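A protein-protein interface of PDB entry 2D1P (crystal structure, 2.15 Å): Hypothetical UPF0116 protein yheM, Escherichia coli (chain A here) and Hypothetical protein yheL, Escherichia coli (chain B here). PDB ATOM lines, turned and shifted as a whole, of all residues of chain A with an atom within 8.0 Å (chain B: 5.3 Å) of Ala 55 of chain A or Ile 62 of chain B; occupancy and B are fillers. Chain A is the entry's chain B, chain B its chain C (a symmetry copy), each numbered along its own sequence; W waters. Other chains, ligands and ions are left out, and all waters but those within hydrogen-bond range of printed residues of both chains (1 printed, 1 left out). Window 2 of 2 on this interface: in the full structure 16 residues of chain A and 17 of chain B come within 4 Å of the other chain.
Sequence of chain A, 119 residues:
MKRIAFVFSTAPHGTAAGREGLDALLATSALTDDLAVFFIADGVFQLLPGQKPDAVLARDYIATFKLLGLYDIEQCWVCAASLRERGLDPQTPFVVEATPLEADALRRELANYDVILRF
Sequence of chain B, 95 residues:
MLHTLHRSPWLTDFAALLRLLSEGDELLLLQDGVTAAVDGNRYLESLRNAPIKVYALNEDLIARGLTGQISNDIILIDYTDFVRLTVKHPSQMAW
Of chain B, only Glu 59 and Ile 62 come within 4 Å of Ala 55 of chain A.
Of the printed residues of chain A, Ile 62 of chain B touches Gln 51, Lys 52 and Ala 55.
Of chain A, only His 13 (3.0 Å), Gln 51 (3.3 Å), Lys 52 (3.5 Å), Pro 53 (3.7 Å) and Val 56 (3.7 Å) come within 4 Å of Ala 63 of chain B.
Of the printed residues of chain B, Lys 52 of chain A touches Ile 62 and Ala 63.
Of the printed residues of chain A, Arg 64 of chain B touches His 13 (3.7 Å) and Gln 51 (3.6 Å).
Of the printed residues of chain B, Pro 53 of chain A touches Ala 63 (3.7 Å).
Printed residues of chain A within 4 Å of Gly 65 of chain B: Gln 51 (3.8 Å).
The nearest residue of chain B that does not touch Ala 55 of chain A is Ala 63 of chain B (4.7 Å).
The nearest residue of chain A that does not touch Ile 62 of chain B is Gly 50 of chain A (4.2 Å).
The nearest printed residue of chain A that does not touch Arg 64 of chain B is Lys 52 of chain A (4.9 Å).
Among the printed residues, pairs that only touch across the chains: His 13 of chain A with Arg 64 of chain B (3.7 Å), Gln 51 of chain A with Ile 62 of chain B (3.97 Å), Gln 51 of chain A with Ala 63 of chain B (3.3 Å), Gln 51 of chain A with Arg 64 of chain B (3.6 Å), Gln 51 of chain A with Gly 65 of chain B (3.8 Å), Lys 52 of chain A with Ala 63 of chain B (3.5 Å), Pro 53 of chain A with Ala 63 of chain B (3.7 Å), Ala 55 of chain A with Glu 59 of chain B (3.8 Å), Ala 55 of chain A with Ile 62 of chain B (3.98 Å), Val 56 of chain A with Glu 59 of chain B (3.6 Å), Val 56 of chain A with Asp 60 of chain B (3.3 Å) and Val 56 of chain A with Ala 63 of chain B (3.7 Å).
A ring nitrogen (NE2) of His 13 of chain A lies within hydrogen-bond range of the side-chain amide oxygen (OE1) of Gln 51 of chain A (2.7 Å).
The backbone carbonyl oxygen (O) of Pro 53 of chain A lies within hydrogen-bond range of the backbone NH (N) of Ala 58 of chain A.
OE2 of Glu 59 of chain B is in hydrogen-bond range of N of Tyr 79 of chain B (3.2 Å).
The side-chain carboxylate (OD1) of Asp 60 of chain B lies within salt-bridge range of the guanidinium group (NH1) of Arg 64 of chain B (3.0 Å).
NE2 of His 13 of chain A is in hydrogen-bond range of O of Ala 63 of chain B.
O of Ile 62 of chain B sits at hydrogen-bond distance from N of Lys 52 of chain A, at 3.1 Å.
Water W1 lies within hydrogen-bond range of O of Gly 50 of chain A (2.6 Å) and O of Ile 62 of chain B (2.7 Å).
Hydrophobic or aromatic side chains of chain A that line the printed part of chain B: His 13, Pro 53, Ala 55 and Val 56.
Of the 11 printed residues of chain B, 6 touch a printed residue of chain A.
Hydrophobic or aromatic side chains of chain B within 4 Å of the printed part of chain A: Ile 62 and Ala 63.
Among the printed residues, 14 pairs touch across the chains.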
ATOM      1  N   HIS A  13      30.055 -23.551 -22.809  1.00  0.00           N
ATOM      2  CA  HIS A  13      30.306 -23.351 -21.387  1.00  0.00           C
ATOM      3  C   HIS A  13      31.703 -23.676 -20.832  1.00  0.00           C
ATOM      4  O   HIS A  13      32.246 -22.901 -20.036  1.00  0.00           O
ATOM      5  CB  HIS A  13      29.212 -24.092 -20.613  1.00  0.00           C
ATOM      6  CG  HIS A  13      27.871 -24.016 -21.280  1.00  0.00           C
ATOM      7  ND1 HIS A  13      27.305 -22.822 -21.674  1.00  0.00           N
ATOM      8  CD2 HIS A  13      27.011 -24.987 -21.671  1.00  0.00           C
ATOM      9  CE1 HIS A  13      26.155 -23.061 -22.280  1.00  0.00           C
ATOM     10  NE2 HIS A  13      25.953 -24.367 -22.290  1.00  0.00           N
ATOM     11  N   PRO A  49      19.051 -28.138 -27.332  1.00  0.00           N
ATOM     12  CA  PRO A  49      18.004 -27.372 -26.651  1.00  0.00           C
ATOM     13  C   PRO A  49      17.940 -27.723 -25.166  1.00  0.00           C
ATOM     14  O   PRO A  49      18.487 -28.735 -24.737  1.00  0.00           O
ATOM     15  CB  PRO A  49      16.741 -27.787 -27.402  1.00  0.00           C
ATOM     16  CG  PRO A  49      17.005 -29.236 -27.670  1.00  0.00           C
ATOM     17  CD  PRO A  49      18.459 -29.224 -28.141  1.00  0.00           C
ATOM     18  N   GLY A  50      17.286 -26.877 -24.379  1.00  0.00           N
ATOM     19  CA  GLY A  50      17.157 -27.142 -22.956  1.00  0.00           C
ATOM     20  C   GLY A  50      18.398 -26.934 -22.101  1.00  0.00           C
ATOM     21  O   GLY A  50      18.419 -27.338 -20.942  1.00  0.00           O
ATOM     22  N   GLN A  51      19.436 -26.318 -22.656  1.00  0.00           N
ATOM     23  CA  GLN A  51      20.648 -26.070 -21.878  1.00  0.00           C
ATOM     24  C   GLN A  51      20.373 -25.040 -20.778  1.00  0.00           C
ATOM     25  O   GLN A  51      19.693 -24.038 -21.004  1.00  0.00           O
ATOM     26  CB  GLN A  51      21.762 -25.553 -22.788  1.00  0.00           C
ATOM     27  CG  GLN A  51      22.190 -26.523 -23.869  1.00  0.00           C
ATOM     28  CD  GLN A  51      23.353 -25.992 -24.673  1.00  0.00           C
ATOM     29  OE1 GLN A  51      24.405 -25.669 -24.119  1.00  0.00           O
ATOM     30  NE2 GLN A  51      23.175 -25.893 -25.983  1.00  0.00           N
ATOM     31  N   LYS A  52      20.903 -25.283 -19.588  1.00  0.00           N
ATOM     32  CA  LYS A  52      20.708 -24.361 -18.477  1.00  0.00           C
ATOM     33  C   LYS A  52      22.043 -24.109 -17.778  1.00  0.00           C
ATOM     34  O   LYS A  52      22.272 -24.564 -16.658  1.00  0.00           O
ATOM     35  CB  LYS A  52      19.680 -24.938 -17.501  1.00  0.00           C
ATOM     36  CG  LYS A  52      18.321 -25.191 -18.153  1.00  0.00           C
ATOM     37  CD  LYS A  52      17.190 -25.222 -17.129  1.00  0.00           C
ATOM     38  CE  LYS A  52      15.827 -25.228 -17.823  1.00  0.00           C
ATOM     39  NZ  LYS A  52      14.689 -25.024 -16.877  1.00  0.00           N
ATOM     40  N   PRO A  53      22.936 -23.354 -18.438  1.00  0.00           N
ATOM     41  CA  PRO A  53      24.268 -23.028 -17.916  1.00  0.00           C
ATOM     42  C   PRO A  53      24.364 -22.280 -16.590  1.00  0.00           C
ATOM     43  O   PRO A  53      25.427 -22.278 -15.963  1.00  0.00           O
ATOM     44  CB  PRO A  53      24.920 -22.269 -19.073  1.00  0.00           C
ATOM     45  CG  PRO A  53      23.760 -21.634 -19.762  1.00  0.00           C
ATOM     46  CD  PRO A  53      22.722 -22.728 -19.754  1.00  0.00           C
ATOM     47  N   ASP A  54      23.284 -21.643 -16.147  1.00  0.00           N
ATOM     48  CA  ASP A  54      23.347 -20.928 -14.878  1.00  0.00           C
ATOM     49  C   ASP A  54      23.679 -21.921 -13.763  1.00  0.00           C
ATOM     50  O   ASP A  54      24.136 -21.535 -12.689  1.00  0.00           O
ATOM     51  CB  ASP A  54      22.023 -20.207 -14.589  1.00  0.00           C
ATOM     52  CG  ASP A  54      20.840 -21.151 -14.520  1.00  0.00           C
ATOM     53  OD1 ASP A  54      19.689 -20.658 -14.428  1.00  0.00           O
ATOM     54  OD2 ASP A  54      21.053 -22.384 -14.555  1.00  0.00           O
ATOM     55  N   ALA A  55      23.458 -23.205 -14.040  1.00  0.00           N
ATOM     56  CA  ALA A  55      23.744 -24.267 -13.082  1.00  0.00           C
ATOM     57  C   ALA A  55      25.232 -24.280 -12.755  1.00  0.00           C
ATOM     58  O   ALA A  55      25.634 -24.687 -11.670  1.00  0.00           O
ATOM     59  CB  ALA A  55      23.319 -25.623 -13.656  1.00  0.00           C
ATOM     60  N   VAL A  56      26.050 -23.840 -13.704  1.00  0.00           N
ATOM     61  CA  VAL A  56      27.487 -23.794 -13.486  1.00  0.00           C
ATOM     62  C   VAL A  56      28.005 -22.359 -13.554  1.00  0.00           C
ATOM     63  O   VAL A  56      29.169 -22.121 -13.874  1.00  0.00           O
ATOM     64  CB  VAL A  56      28.240 -24.685 -14.504  1.00  0.00           C
ATOM     65  CG1 VAL A  56      27.850 -26.139 -14.299  1.00  0.00           C
ATOM     66  CG2 VAL A  56      27.935 -24.247 -15.926  1.00  0.00           C
ATOM     67  N   LEU A  57      27.118 -21.410 -13.256  1.00  0.00           N
ATOM     68  CA  LEU A  57      27.451 -19.983 -13.235  1.00  0.00           C
ATOM     69  C   LEU A  57      27.928 -19.412 -14.570  1.00  0.00           C
ATOM     70  O   LEU A  57      28.660 -18.417 -14.604  1.00  0.00           O
ATOM     71  CB  LEU A  57      28.513 -19.723 -12.159  1.00  0.00           C
ATOM     72  CG  LEU A  57      28.249 -20.396 -10.806  1.00  0.00           C
ATOM     73  CD1 LEU A  57      29.379 -20.070  -9.838  1.00  0.00           C
ATOM     74  CD2 LEU A  57      26.911 -19.918 -10.253  1.00  0.00           C
ATOM     75  N   ALA A  58      27.503 -20.031 -15.666  1.00  0.00           N
ATOM     76  CA  ALA A  58      27.882 -19.577 -17.000  1.00  0.00           C
ATOM     77  C   ALA A  58      26.702 -18.858 -17.662  1.00  0.00           C
ATOM     78  O   ALA A  58      25.536 -19.146 -17.370  1.00  0.00           O
ATOM     79  CB  ALA A  58      28.316 -20.767 -17.852  1.00  0.00           C
ATOM     80  N   ARG A  59      27.001 -17.922 -18.553  1.00  0.00           N
ATOM     81  CA  ARG A  59      25.938 -17.181 -19.215  1.00  0.00           C
ATOM     82  C   ARG A  59      25.117 -18.030 -20.178  1.00  0.00           C
ATOM     83  O   ARG A  59      25.668 -18.810 -20.954  1.00  0.00           O
ATOM     84  CB  ARG A  59      26.511 -15.997 -19.991  1.00  0.00           C
ATOM     85  CG  ARG A  59      25.440 -15.176 -20.700  1.00  0.00           C
ATOM     86  CD  ARG A  59      26.023 -14.182 -21.684  1.00  0.00           C
ATOM     87  NE  ARG A  59      24.983 -13.287 -22.187  1.00  0.00           N
ATOM     88  CZ  ARG A  59      24.528 -12.225 -21.530  1.00  0.00           C
ATOM     89  NH1 ARG A  59      25.026 -11.906 -20.337  1.00  0.00           N
ATOM     90  NH2 ARG A  59      23.565 -11.481 -22.058  1.00  0.00           N
ATOM     91  N   ASN B  58      26.386 -33.868 -12.517  1.00  0.00           N
ATOM     92  CA  ASN B  58      25.050 -33.510 -12.979  1.00  0.00           C
ATOM     93  C   ASN B  58      24.899 -32.042 -13.371  1.00  0.00           C
ATOM     94  O   ASN B  58      24.245 -31.721 -14.366  1.00  0.00           O
ATOM     95  CB  ASN B  58      24.023 -33.866 -11.900  1.00  0.00           C
ATOM     96  CG  ASN B  58      22.603 -33.792 -12.409  1.00  0.00           C
ATOM     97  OD1 ASN B  58      22.281 -34.354 -13.453  1.00  0.00           O
ATOM     98  ND2 ASN B  58      21.744 -33.103 -11.671  1.00  0.00           N
ATOM     99  N   GLU B  59      25.497 -31.151 -12.586  1.00  0.00           N
ATOM    100  CA  GLU B  59      25.416 -29.726 -12.870  1.00  0.00           C
ATOM    101  C   GLU B  59      25.872 -29.419 -14.295  1.00  0.00           C
ATOM    102  O   GLU B  59      25.254 -28.611 -14.986  1.00  0.00           O
ATOM    103  CB  GLU B  59      26.249 -28.925 -11.854  1.00  0.00           C
ATOM    104  CG  GLU B  59      25.618 -28.836 -10.456  1.00  0.00           C
ATOM    105  CD  GLU B  59      25.885 -30.061  -9.581  1.00  0.00           C
ATOM    106  OE1 GLU B  59      26.302 -31.114 -10.109  1.00  0.00           O
ATOM    107  OE2 GLU B  59      25.669 -29.966  -8.354  1.00  0.00           O
ATOM    108  N   ASP B  60      26.944 -30.072 -14.735  1.00  0.00           N
ATOM    109  CA  ASP B  60      27.462 -29.858 -16.081  1.00  0.00           C
ATOM    110  C   ASP B  60      26.616 -30.501 -17.184  1.00  0.00           C
ATOM    111  O   ASP B  60      26.633 -30.043 -18.329  1.00  0.00           O
ATOM    112  CB  ASP B  60      28.910 -30.344 -16.177  1.00  0.00           C
ATOM    113  CG  ASP B  60      29.883 -29.388 -15.504  1.00  0.00           C
ATOM    114  OD1 ASP B  60      29.894 -28.193 -15.878  1.00  0.00           O
ATOM    115  OD2 ASP B  60      30.625 -29.822 -14.603  1.00  0.00           O
ATOM    116  N   LEU B  61      25.894 -31.569 -16.856  1.00  0.00           N
ATOM    117  CA  LEU B  61      25.032 -32.201 -17.854  1.00  0.00           C
ATOM    118  C   LEU B  61      23.834 -31.263 -18.040  1.00  0.00           C
ATOM    119  O   LEU B  61      23.365 -31.039 -19.156  1.00  0.00           O
ATOM    120  CB  LEU B  61      24.573 -33.583 -17.377  1.00  0.00           C
ATOM    121  CG  LEU B  61      25.695 -34.624 -17.291  1.00  0.00           C
ATOM    122  CD1 LEU B  61      25.220 -35.833 -16.530  1.00  0.00           C
ATOM    123  CD2 LEU B  61      26.165 -35.011 -18.699  1.00  0.00           C
ATOM    124  N   ILE B  62      23.366 -30.693 -16.934  1.00  0.00           N
ATOM    125  CA  ILE B  62      22.243 -29.764 -16.966  1.00  0.00           C
ATOM    126  C   ILE B  62      22.604 -28.524 -17.789  1.00  0.00           C
ATOM    127  O   ILE B  62      21.797 -28.028 -18.578  1.00  0.00           O
ATOM    128  CB  ILE B  62      21.851 -29.332 -15.539  1.00  0.00           C
ATOM    129  CG1 ILE B  62      21.219 -30.519 -14.805  1.00  0.00           C
ATOM    130  CG2 ILE B  62      20.911 -28.130 -15.587  1.00  0.00           C
ATOM    131  CD1 ILE B  62      20.872 -30.228 -13.344  1.00  0.00           C
ATOM    132  N   ALA B  63      23.828 -28.037 -17.607  1.00  0.00           N
ATOM    133  CA  ALA B  63      24.303 -26.857 -18.318  1.00  0.00           C
ATOM    134  C   ALA B  63      24.371 -27.083 -19.823  1.00  0.00           C
ATOM    135  O   ALA B  63      24.155 -26.165 -20.609  1.00  0.00           O
ATOM    136  CB  ALA B  63      25.686 -26.462 -17.798  1.00  0.00           C
ATOM    137  N   ARG B  64      24.671 -28.316 -20.212  1.00  0.00           N
ATOM    138  CA  ARG B  64      24.802 -28.669 -21.614  1.00  0.00           C
ATOM    139  C   ARG B  64      23.597 -29.395 -22.227  1.00  0.00           C
ATOM    140  O   ARG B  64      23.658 -29.840 -23.376  1.00  0.00           O
ATOM    141  CB  ARG B  64      26.073 -29.501 -21.780  1.00  0.00           C
ATOM    142  CG  ARG B  64      27.327 -28.708 -21.431  1.00  0.00           C
ATOM    143  CD  ARG B  64      28.529 -29.604 -21.225  1.00  0.00           C
ATOM    144  NE  ARG B  64      29.734 -28.831 -20.935  1.00  0.00           N
ATOM    145  CZ  ARG B  64      29.977 -28.213 -19.781  1.00  0.00           C
ATOM    146  NH1 ARG B  64      29.097 -28.272 -18.786  1.00  0.00           N
ATOM    147  NH2 ARG B  64      31.105 -27.531 -19.629  1.00  0.00           N
ATOM    148  N   GLY B  65      22.508 -29.500 -21.465  1.00  0.00           N
ATOM    149  CA  GLY B  65      21.307 -30.167 -21.953  1.00  0.00           C
ATOM    150  C   GLY B  65      21.525 -31.623 -22.341  1.00  0.00           C
ATOM    151  O   GLY B  65      21.055 -32.071 -23.385  1.00  0.00           O
ATOM    152  N   LEU B  66      22.216 -32.374 -21.490  1.00  0.00           N
ATOM    153  CA  LEU B  66      22.503 -33.771 -21.783  1.00  0.00           C
ATOM    154  C   LEU B  66      21.979 -34.759 -20.747  1.00  0.00           C
ATOM    155  O   LEU B  66      22.245 -35.954 -20.845  1.00  0.00           O
ATOM    156  CB  LEU B  66      24.014 -33.948 -21.930  1.00  0.00           C
ATOM    157  CG  LEU B  66      24.662 -33.221 -23.108  1.00  0.00           C
ATOM    158  CD1 LEU B  66      26.173 -33.246 -22.957  1.00  0.00           C
ATOM    159  CD2 LEU B  66      24.238 -33.891 -24.414  1.00  0.00           C
ATOM    160  N   THR B  67      21.223 -34.269 -19.770  1.00  0.00           N
ATOM    161  CA  THR B  67      20.697 -35.119 -18.702  1.00  0.00           C
ATOM    162  C   THR B  67      19.921 -36.368 -19.130  1.00  0.00           C
ATOM    163  O   THR B  67      19.898 -37.368 -18.409  1.00  0.00           O
ATOM    164  CB  THR B  67      19.807 -34.307 -17.728  1.00  0.00           C
ATOM    165  OG1 THR B  67      18.832 -33.571 -18.471  1.00  0.00           O
ATOM    166  CG2 THR B  67      20.655 -33.342 -16.899  1.00  0.00           C
ATOM    167  N   TYR B  79      27.750 -31.733  -6.707  1.00  0.00           N
ATOM    168  CA  TYR B  79      28.977 -31.203  -6.126  1.00  0.00           C
ATOM    169  C   TYR B  79      29.307 -31.819  -4.771  1.00  0.00           C
ATOM    170  O   TYR B  79      30.471 -32.095  -4.479  1.00  0.00           O
ATOM    171  CB  TYR B  79      28.889 -29.680  -6.015  1.00  0.00           C
ATOM    172  CG  TYR B  79      29.348 -28.973  -7.266  1.00  0.00           C
ATOM    173  CD1 TYR B  79      30.688 -29.009  -7.658  1.00  0.00           C
ATOM    174  CD2 TYR B  79      28.450 -28.260  -8.059  1.00  0.00           C
ATOM    175  CE1 TYR B  79      31.123 -28.347  -8.805  1.00  0.00           C
ATOM    176  CE2 TYR B  79      28.876 -27.595  -9.209  1.00  0.00           C
ATOM    177  CZ  TYR B  79      30.211 -27.640  -9.572  1.00  0.00           C
ATOM    178  OH  TYR B  79      30.636 -26.954 -10.687  1.00  0.00           O
HETATM  179  O   HOH W   1      19.289 -28.912 -19.076  1.00  0.00           O
